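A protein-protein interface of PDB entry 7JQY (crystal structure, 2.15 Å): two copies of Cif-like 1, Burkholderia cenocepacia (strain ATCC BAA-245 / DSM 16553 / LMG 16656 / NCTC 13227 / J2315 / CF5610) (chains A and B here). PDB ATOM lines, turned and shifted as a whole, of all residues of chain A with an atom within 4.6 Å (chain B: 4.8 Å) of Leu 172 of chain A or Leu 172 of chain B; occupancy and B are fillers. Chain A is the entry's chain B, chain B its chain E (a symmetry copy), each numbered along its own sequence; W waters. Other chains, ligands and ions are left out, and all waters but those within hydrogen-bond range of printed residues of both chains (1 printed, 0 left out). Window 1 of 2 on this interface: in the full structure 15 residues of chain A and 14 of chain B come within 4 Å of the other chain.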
ATOM      1  N   TRP A 168       5.202   4.317   3.859  1.00  0.00           N
ATOM      2  CA  TRP A 168       5.844   3.006   3.862  1.00  0.00           C
ATOM      3  C   TRP A 168       4.819   1.877   3.841  1.00  0.00           C
ATOM      4  O   TRP A 168       5.077   0.807   3.276  1.00  0.00           O
ATOM      5  CB  TRP A 168       6.737   2.863   5.099  1.00  0.00           C
ATOM      6  CG  TRP A 168       5.962   2.714   6.394  1.00  0.00           C
ATOM      7  CD1 TRP A 168       5.625   3.708   7.270  1.00  0.00           C
ATOM      8  CD2 TRP A 168       5.418   1.499   6.941  1.00  0.00           C
ATOM      9  NE1 TRP A 168       4.906   3.190   8.325  1.00  0.00           N
ATOM     10  CE2 TRP A 168       4.763   1.840   8.147  1.00  0.00           C
ATOM     11  CE3 TRP A 168       5.415   0.162   6.527  1.00  0.00           C
ATOM     12  CZ2 TRP A 168       4.124   0.892   8.943  1.00  0.00           C
ATOM     13  CZ3 TRP A 168       4.771  -0.780   7.320  1.00  0.00           C
ATOM     14  CH2 TRP A 168       4.138  -0.409   8.515  1.00  0.00           C
ATOM     15  N   HIS A 169       3.653   2.104   4.446  1.00  0.00           N
ATOM     16  CA  HIS A 169       2.662   1.061   4.652  1.00  0.00           C
ATOM     17  C   HIS A 169       1.845   0.759   3.404  1.00  0.00           C
ATOM     18  O   HIS A 169       1.107  -0.232   3.400  1.00  0.00           O
ATOM     19  CB  HIS A 169       1.746   1.456   5.816  1.00  0.00           C
ATOM     20  CG  HIS A 169       0.993   2.728   5.586  1.00  0.00           C
ATOM     21  ND1 HIS A 169       1.608   3.961   5.527  1.00  0.00           N
ATOM     22  CD2 HIS A 169      -0.331   2.956   5.404  1.00  0.00           C
ATOM     23  CE1 HIS A 169       0.697   4.893   5.307  1.00  0.00           C
ATOM     24  NE2 HIS A 169      -0.489   4.310   5.229  1.00  0.00           N
ATOM     25  N   PHE A 170       1.944   1.587   2.362  1.00  0.00           N
ATOM     26  CA  PHE A 170       1.243   1.304   1.115  1.00  0.00           C
ATOM     27  C   PHE A 170       1.630  -0.070   0.581  1.00  0.00           C
ATOM     28  O   PHE A 170       0.772  -0.849   0.147  1.00  0.00           O
ATOM     29  CB  PHE A 170       1.554   2.381   0.071  1.00  0.00           C
ATOM     30  CG  PHE A 170       0.772   3.658   0.246  1.00  0.00           C
ATOM     31  CD1 PHE A 170       0.239   4.006   1.478  1.00  0.00           C
ATOM     32  CD2 PHE A 170       0.576   4.513  -0.826  1.00  0.00           C
ATOM     33  CE1 PHE A 170      -0.479   5.181   1.634  1.00  0.00           C
ATOM     34  CE2 PHE A 170      -0.143   5.685  -0.677  1.00  0.00           C
ATOM     35  CZ  PHE A 170      -0.671   6.020   0.554  1.00  0.00           C
ATOM     36  N   GLY A 171       2.930  -0.375   0.586  1.00  0.00           N
ATOM     37  CA  GLY A 171       3.371  -1.675   0.108  1.00  0.00           C
ATOM     38  C   GLY A 171       2.785  -2.827   0.908  1.00  0.00           C
ATOM     39  O   GLY A 171       2.186  -3.746   0.345  1.00  0.00           O
ATOM     40  N   LEU A 172       2.962  -2.798   2.233  1.00  0.00           N
ATOM     41  CA  LEU A 172       2.481  -3.892   3.072  1.00  0.00           C
ATOM     42  C   LEU A 172       0.978  -4.074   2.928  1.00  0.00           C
ATOM     43  O   LEU A 172       0.492  -5.193   2.750  1.00  0.00           O
ATOM     44  CB  LEU A 172       2.850  -3.643   4.536  1.00  0.00           C
ATOM     45  CG  LEU A 172       2.163  -4.598   5.518  1.00  0.00           C
ATOM     46  CD1 LEU A 172       2.637  -6.025   5.296  1.00  0.00           C
ATOM     47  CD2 LEU A 172       2.379  -4.177   6.969  1.00  0.00           C
ATOM     48  N   HIS A 173       0.222  -2.980   3.014  1.00  0.00           N
ATOM     49  CA  HIS A 173      -1.226  -3.087   2.932  1.00  0.00           C
ATOM     50  C   HIS A 173      -1.668  -3.641   1.590  1.00  0.00           C
ATOM     51  O   HIS A 173      -2.740  -4.245   1.492  1.00  0.00           O
ATOM     52  CB  HIS A 173      -1.867  -1.730   3.185  1.00  0.00           C
ATOM     53  CG  HIS A 173      -1.759  -1.279   4.605  1.00  0.00           C
ATOM     54  ND1 HIS A 173      -2.458  -0.200   5.097  1.00  0.00           N
ATOM     55  CD2 HIS A 173      -1.029  -1.762   5.639  1.00  0.00           C
ATOM     56  CE1 HIS A 173      -2.160  -0.033   6.374  1.00  0.00           C
ATOM     57  NE2 HIS A 173      -1.299  -0.970   6.728  1.00  0.00           N
ATOM     58  N   GLN A 174      -0.853  -3.475   0.553  1.00  0.00           N
ATOM     59  CA  GLN A 174      -1.234  -3.984  -0.755  1.00  0.00           C
ATOM     60  C   GLN A 174      -0.885  -5.452  -0.947  1.00  0.00           C
ATOM     61  O   GLN A 174      -1.203  -6.002  -2.003  1.00  0.00           O
ATOM     62  CB  GLN A 174      -0.593  -3.136  -1.857  1.00  0.00           C
ATOM     63  CG  GLN A 174      -1.332  -1.841  -2.129  1.00  0.00           C
ATOM     64  CD  GLN A 174      -0.537  -0.890  -3.016  1.00  0.00           C
ATOM     65  OE1 GLN A 174       0.654  -1.083  -3.227  1.00  0.00           O
ATOM     66  NE2 GLN A 174      -1.191   0.147  -3.513  1.00  0.00           N
ATOM     67  N   GLN A 175      -0.276  -6.104   0.043  1.00  0.00           N
ATOM     68  CA  GLN A 175       0.017  -7.538  -0.023  1.00  0.00           C
ATOM     69  C   GLN A 175      -1.191  -8.335   0.487  1.00  0.00           C
ATOM     70  O   GLN A 175      -1.400  -8.473   1.697  1.00  0.00           O
ATOM     71  CB  GLN A 175       1.274  -7.859   0.779  1.00  0.00           C
ATOM     72  CG  GLN A 175       2.492  -7.006   0.410  1.00  0.00           C
ATOM     73  CD  GLN A 175       2.748  -6.957  -1.090  1.00  0.00           C
ATOM     74  OE1 GLN A 175       3.109  -7.966  -1.702  1.00  0.00           O
ATOM     75  NE2 GLN A 175       2.544  -5.788  -1.690  1.00  0.00           N
ATOM     76  N   ALA A 179      -0.630  -9.224   4.681  1.00  0.00           N
ATOM     77  CA  ALA A 179      -0.924  -8.156   5.635  1.00  0.00           C
ATOM     78  C   ALA A 179      -1.879  -8.630   6.724  1.00  0.00           C
ATOM     79  O   ALA A 179      -1.664  -8.357   7.915  1.00  0.00           O
ATOM     80  CB  ALA A 179      -1.512  -6.954   4.898  1.00  0.00           C
ATOM     81  N   LEU A 182      -0.085 -11.106   9.075  1.00  0.00           N
ATOM     82  CA  LEU A 182       0.889 -10.496   9.978  1.00  0.00           C
ATOM     83  C   LEU A 182       0.207  -9.691  11.074  1.00  0.00           C
ATOM     84  O   LEU A 182       0.634  -9.725  12.233  1.00  0.00           O
ATOM     85  CB  LEU A 182       1.846  -9.591   9.195  1.00  0.00           C
ATOM     86  CG  LEU A 182       2.821 -10.249   8.226  1.00  0.00           C
ATOM     87  CD1 LEU A 182       3.709  -9.176   7.614  1.00  0.00           C
ATOM     88  CD2 LEU A 182       3.646 -11.303   8.930  1.00  0.00           C
ATOM     89  N   ILE A 183      -0.847  -8.949  10.729  1.00  0.00           N
ATOM     90  CA  ILE A 183      -1.409  -7.983  11.668  1.00  0.00           C
ATOM     91  C   ILE A 183      -2.586  -8.537  12.490  1.00  0.00           C
ATOM     92  O   ILE A 183      -2.889  -7.992  13.563  1.00  0.00           O
ATOM     93  CB  ILE A 183      -1.782  -6.700  10.894  1.00  0.00           C
ATOM     94  CG1 ILE A 183      -0.527  -6.117  10.225  1.00  0.00           C
ATOM     95  CG2 ILE A 183      -2.385  -5.651  11.822  1.00  0.00           C
ATOM     96  CD1 ILE A 183      -0.806  -5.081   9.161  1.00  0.00           C
ATOM     97  N   TYR A 190      -0.306  -2.472  16.333  1.00  0.00           N
ATOM     98  CA  TYR A 190      -0.022  -1.916  15.018  1.00  0.00           C
ATOM     99  C   TYR A 190      -0.646  -0.537  14.853  1.00  0.00           C
ATOM    100  O   TYR A 190       0.014   0.395  14.382  1.00  0.00           O
ATOM    101  CB  TYR A 190      -0.520  -2.869  13.930  1.00  0.00           C
ATOM    102  CG  TYR A 190      -0.212  -2.422  12.509  1.00  0.00           C
ATOM    103  CD1 TYR A 190       1.088  -2.497  11.993  1.00  0.00           C
ATOM    104  CD2 TYR A 190      -1.220  -1.954  11.673  1.00  0.00           C
ATOM    105  CE1 TYR A 190       1.364  -2.117  10.699  1.00  0.00           C
ATOM    106  CE2 TYR A 190      -0.953  -1.561  10.366  1.00  0.00           C
ATOM    107  CZ  TYR A 190       0.343  -1.645   9.884  1.00  0.00           C
ATOM    108  OH  TYR A 190       0.617  -1.254   8.589  1.00  0.00           O
ATOM    109  N   TRP B 168       8.139  -3.810  -2.335  1.00  0.00           N
ATOM    110  CA  TRP B 168       7.113  -3.397  -1.385  1.00  0.00           C
ATOM    111  C   TRP B 168       7.600  -3.545   0.048  1.00  0.00           C
ATOM    112  O   TRP B 168       7.212  -2.767   0.923  1.00  0.00           O
ATOM    113  CB  TRP B 168       5.837  -4.223  -1.597  1.00  0.00           C
ATOM    114  CG  TRP B 168       5.997  -5.627  -1.112  1.00  0.00           C
ATOM    115  CD1 TRP B 168       6.362  -6.712  -1.850  1.00  0.00           C
ATOM    116  CD2 TRP B 168       5.849  -6.087   0.231  1.00  0.00           C
ATOM    117  NE1 TRP B 168       6.440  -7.824  -1.052  1.00  0.00           N
ATOM    118  CE2 TRP B 168       6.127  -7.467   0.231  1.00  0.00           C
ATOM    119  CE3 TRP B 168       5.508  -5.466   1.436  1.00  0.00           C
ATOM    120  CZ2 TRP B 168       6.060  -8.240   1.388  1.00  0.00           C
ATOM    121  CZ3 TRP B 168       5.449  -6.234   2.586  1.00  0.00           C
ATOM    122  CH2 TRP B 168       5.722  -7.605   2.553  1.00  0.00           C
ATOM    123  N   HIS B 169       8.452  -4.532   0.305  1.00  0.00           N
ATOM    124  CA  HIS B 169       8.886  -4.846   1.656  1.00  0.00           C
ATOM    125  C   HIS B 169       9.959  -3.908   2.190  1.00  0.00           C
ATOM    126  O   HIS B 169      10.227  -3.935   3.399  1.00  0.00           O
ATOM    127  CB  HIS B 169       9.427  -6.264   1.701  1.00  0.00           C
ATOM    128  CG  HIS B 169      10.574  -6.493   0.772  1.00  0.00           C
ATOM    129  ND1 HIS B 169      10.457  -6.370  -0.596  1.00  0.00           N
ATOM    130  CD2 HIS B 169      11.858  -6.855   1.008  1.00  0.00           C
ATOM    131  CE1 HIS B 169      11.622  -6.634  -1.162  1.00  0.00           C
ATOM    132  NE2 HIS B 169      12.486  -6.940  -0.211  1.00  0.00           N
ATOM    133  N   PHE B 170      10.577  -3.082   1.341  1.00  0.00           N
ATOM    134  CA  PHE B 170      11.580  -2.156   1.854  1.00  0.00           C
ATOM    135  C   PHE B 170      10.987  -1.313   2.974  1.00  0.00           C
ATOM    136  O   PHE B 170      11.561  -1.218   4.069  1.00  0.00           O
ATOM    137  CB  PHE B 170      12.104  -1.264   0.724  1.00  0.00           C
ATOM    138  CG  PHE B 170      13.159  -1.910  -0.137  1.00  0.00           C
ATOM    139  CD1 PHE B 170      13.304  -3.291  -0.179  1.00  0.00           C
ATOM    140  CD2 PHE B 170      14.018  -1.118  -0.905  1.00  0.00           C
ATOM    141  CE1 PHE B 170      14.278  -3.879  -0.973  1.00  0.00           C
ATOM    142  CE2 PHE B 170      14.998  -1.688  -1.706  1.00  0.00           C
ATOM    143  CZ  PHE B 170      15.139  -3.067  -1.740  1.00  0.00           C
ATOM    144  N   GLY B 171       9.786  -0.770   2.742  1.00  0.00           N
ATOM    145  CA  GLY B 171       9.133   0.050   3.751  1.00  0.00           C
ATOM    146  C   GLY B 171       8.920  -0.684   5.059  1.00  0.00           C
ATOM    147  O   GLY B 171       9.323  -0.207   6.122  1.00  0.00           O
ATOM    148  N   LEU B 172       8.287  -1.863   4.993  1.00  0.00           N
ATOM    149  CA  LEU B 172       8.005  -2.639   6.198  1.00  0.00           C
ATOM    150  C   LEU B 172       9.284  -3.004   6.937  1.00  0.00           C
ATOM    151  O   LEU B 172       9.370  -2.856   8.160  1.00  0.00           O
ATOM    152  CB  LEU B 172       7.218  -3.910   5.844  1.00  0.00           C
ATOM    153  CG  LEU B 172       7.100  -4.966   6.958  1.00  0.00           C
ATOM    154  CD1 LEU B 172       6.370  -4.412   8.177  1.00  0.00           C
ATOM    155  CD2 LEU B 172       6.418  -6.266   6.475  1.00  0.00           C
ATOM    156  N   HIS B 173      10.284  -3.515   6.214  1.00  0.00           N
ATOM    157  CA  HIS B 173      11.512  -3.945   6.875  1.00  0.00           C
ATOM    158  C   HIS B 173      12.202  -2.785   7.590  1.00  0.00           C
ATOM    159  O   HIS B 173      12.970  -3.005   8.532  1.00  0.00           O
ATOM    160  CB  HIS B 173      12.479  -4.562   5.861  1.00  0.00           C
ATOM    161  CG  HIS B 173      12.076  -5.918   5.369  1.00  0.00           C
ATOM    162  ND1 HIS B 173      12.951  -6.757   4.715  1.00  0.00           N
ATOM    163  CD2 HIS B 173      10.899  -6.585   5.442  1.00  0.00           C
ATOM    164  CE1 HIS B 173      12.330  -7.880   4.399  1.00  0.00           C
ATOM    165  NE2 HIS B 173      11.085  -7.803   4.831  1.00  0.00           N
ATOM    166  N   GLN B 174      11.956  -1.552   7.154  1.00  0.00           N
ATOM    167  CA  GLN B 174      12.585  -0.386   7.761  1.00  0.00           C
ATOM    168  C   GLN B 174      11.838   0.155   8.977  1.00  0.00           C
ATOM    169  O   GLN B 174      12.300   1.134   9.577  1.00  0.00           O
ATOM    170  CB  GLN B 174      12.760   0.707   6.706  1.00  0.00           C
ATOM    171  CG  GLN B 174      13.934   0.399   5.779  1.00  0.00           C
ATOM    172  CD  GLN B 174      14.087   1.369   4.620  1.00  0.00           C
ATOM    173  OE1 GLN B 174      13.137   2.034   4.210  1.00  0.00           O
ATOM    174  NE2 GLN B 174      15.312   1.464   4.093  1.00  0.00           N
ATOM    175  N   GLN B 175      10.710  -0.453   9.357  1.00  0.00           N
ATOM    176  CA  GLN B 175       9.966  -0.066  10.556  1.00  0.00           C
ATOM    177  C   GLN B 175      10.549  -0.832  11.733  1.00  0.00           C
ATOM    178  O   GLN B 175      10.184  -1.993  11.974  1.00  0.00           O
ATOM    179  CB  GLN B 175       8.478  -0.375  10.393  1.00  0.00           C
ATOM    180  CG  GLN B 175       7.843   0.244   9.160  1.00  0.00           C
ATOM    181  CD  GLN B 175       8.235   1.699   9.009  1.00  0.00           C
ATOM    182  OE1 GLN B 175       7.918   2.517   9.868  1.00  0.00           O
ATOM    183  NE2 GLN B 175       8.924   2.031   7.913  1.00  0.00           N
ATOM    184  N   ALA B 179       8.252  -4.294  12.397  1.00  0.00           N
ATOM    185  CA  ALA B 179       8.428  -5.436  11.504  1.00  0.00           C
ATOM    186  C   ALA B 179       8.675  -6.715  12.292  1.00  0.00           C
ATOM    187  O   ALA B 179       8.149  -7.782  11.949  1.00  0.00           O
ATOM    188  CB  ALA B 179       9.583  -5.183  10.535  1.00  0.00           C
ATOM    189  N   LEU B 182       5.451  -8.027  13.969  1.00  0.00           N
ATOM    190  CA  LEU B 182       4.497  -8.627  13.051  1.00  0.00           C
ATOM    191  C   LEU B 182       4.954 -10.005  12.586  1.00  0.00           C
ATOM    192  O   LEU B 182       4.129 -10.909  12.418  1.00  0.00           O
ATOM    193  CB  LEU B 182       4.275  -7.714  11.850  1.00  0.00           C
ATOM    194  CG  LEU B 182       3.572  -6.369  12.024  1.00  0.00           C
ATOM    195  CD1 LEU B 182       3.269  -5.794  10.651  1.00  0.00           C
ATOM    196  CD2 LEU B 182       2.294  -6.497  12.842  1.00  0.00           C
ATOM    197  N   ILE B 183       6.253 -10.182  12.334  1.00  0.00           N
ATOM    198  CA  ILE B 183       6.722 -11.392  11.665  1.00  0.00           C
ATOM    199  C   ILE B 183       7.208 -12.475  12.625  1.00  0.00           C
ATOM    200  O   ILE B 183       7.204 -13.658  12.248  1.00  0.00           O
ATOM    201  CB  ILE B 183       7.815 -11.039  10.627  1.00  0.00           C
ATOM    202  CG1 ILE B 183       7.240 -10.090   9.576  1.00  0.00           C
ATOM    203  CG2 ILE B 183       8.336 -12.282   9.901  1.00  0.00           C
ATOM    204  CD1 ILE B 183       8.289  -9.213   8.894  1.00  0.00           C
ATOM    205  N   TYR B 190       6.033 -16.179   6.166  1.00  0.00           N
ATOM    206  CA  TYR B 190       6.477 -14.955   5.498  1.00  0.00           C
ATOM    207  C   TYR B 190       7.591 -15.248   4.490  1.00  0.00           C
ATOM    208  O   TYR B 190       7.550 -14.765   3.351  1.00  0.00           O
ATOM    209  CB  TYR B 190       6.933 -13.934   6.547  1.00  0.00           C
ATOM    210  CG  TYR B 190       7.324 -12.563   6.021  1.00  0.00           C
ATOM    211  CD1 TYR B 190       6.361 -11.660   5.578  1.00  0.00           C
ATOM    212  CD2 TYR B 190       8.662 -12.153   6.011  1.00  0.00           C
ATOM    213  CE1 TYR B 190       6.722 -10.395   5.110  1.00  0.00           C
ATOM    214  CE2 TYR B 190       9.030 -10.895   5.548  1.00  0.00           C
ATOM    215  CZ  TYR B 190       8.060 -10.020   5.097  1.00  0.00           C
ATOM    216  OH  TYR B 190       8.430  -8.766   4.637  1.00  0.00           O
HETATM  217  O   HOH W   1       5.973  -1.882   3.254  1.00  0.00           O
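Trp 168 of chain A touches Gly 171 of chain B, and with the chains exchanged Gly 171 of chain A touches Trp 168 of chain B. Trp 168 of chain A touches Leu 172 of chain B, and with the chains exchanged Leu 172 of chain A touches Trp 168 of chain B. Leu 172 of chain A touches its own counterpart, Leu 172 of chain B. Leu 182 of chain A touches its own counterpart, Leu 182 of chain B. Positions printed for both chains: 168, 169, 170, 171, 172, 173, 174, 175, 179, 182, 183 and 190.
The side-chain amide oxygen of Gln 175 of chain B sits at hydrogen-bond distance from the indole nitrogen of Trp 168 of chain A, at 3.5 Å. The indole nitrogen of Trp 168 of chain B is in hydrogen-bond range of the side-chain amide oxygen of Gln 175 of chain A, at 3.4 Å.
Water W1 lies within hydrogen-bond range of the backbone carbonyl oxygen of Trp 168 of chain B (2.8 Å), the backbone carbonyl oxygen of Trp 168 of chain A (2.8 Å), the backbone NH of Leu 172 of chain B (2.9 Å) and the backbone NH of Leu 172 of chain A (3.3 Å).
Printed residues of chain B within 4 Å of Trp 168 of chain A: Gly 171 (3.9 Å), Leu 172 (3.8 Å) and Gln 175 (3.4 Å). Printed residues of chain A within 4 Å of Trp 168 of chain B: Gly 171 (3.8 Å), Leu 172 (3.8 Å) and Gln 175 (3.4 Å). Phe 170 of chain B touches none of the printed residues of chain A. Printed residues of chain A within 4 Å of Gly 171 of chain B: Trp 168 (3.9 Å). Of the printed residues of chain A, Leu 172 of chain B touches Trp 168 (3.8 Å) and Leu 172 (3.97 Å). Of the printed residues of chain A, Leu 182 of chain B touches Leu 182 and Ile 183. Printed residues of chain A within 4 Å of Ile 183 of chain B: Leu 182 (3.8 Å). The nearest residue of chain B that does not touch Leu 172 of chain A is Leu 182 of chain B (4.1 Å). The nearest residue of chain A that does not touch Leu 172 of chain B is Leu 182 of chain A (4.1 Å). The nearest printed residue of chain A that does not touch Leu 182 of chain B is Leu 172 of chain A (4.1 Å).
Of the 12 printed residues of chain B, 6 touch a printed residue of chain A. Among the printed residues, 10 pairs touch across the chains. Among the printed residues, no Asp or Glu carboxylate lies within 4 Å of a Lys or Arg side-chain nitrogen of the other chain.
The side-chain amide nitrogen (NE2) of Gln 175 of chain A is in hydrogen-bond range of the backbone carbonyl oxygen (O) of Gly 171 of chain A, 2.9 Å away. O of Gly 171 of chain B sits at hydrogen-bond distance from NE2 of Gln 175 of chain B (2.9 Å).
Among the printed residues, merely in contact across the chains: Trp 168 of chain A with Gly 171 of chain B, Trp 168 of chain A with Leu 172 of chain B, Gly 171 of chain A with Trp 168 of chain B, Leu 172 of chain A with Trp 168 of chain B, Leu 172 of chain A with Leu 172 of chain B, Leu 182 of chain A with Leu 182 of chain B, Leu 182 of chain A with Ile 183 of chain B and Ile 183 of chain A with Leu 182 of chain B.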
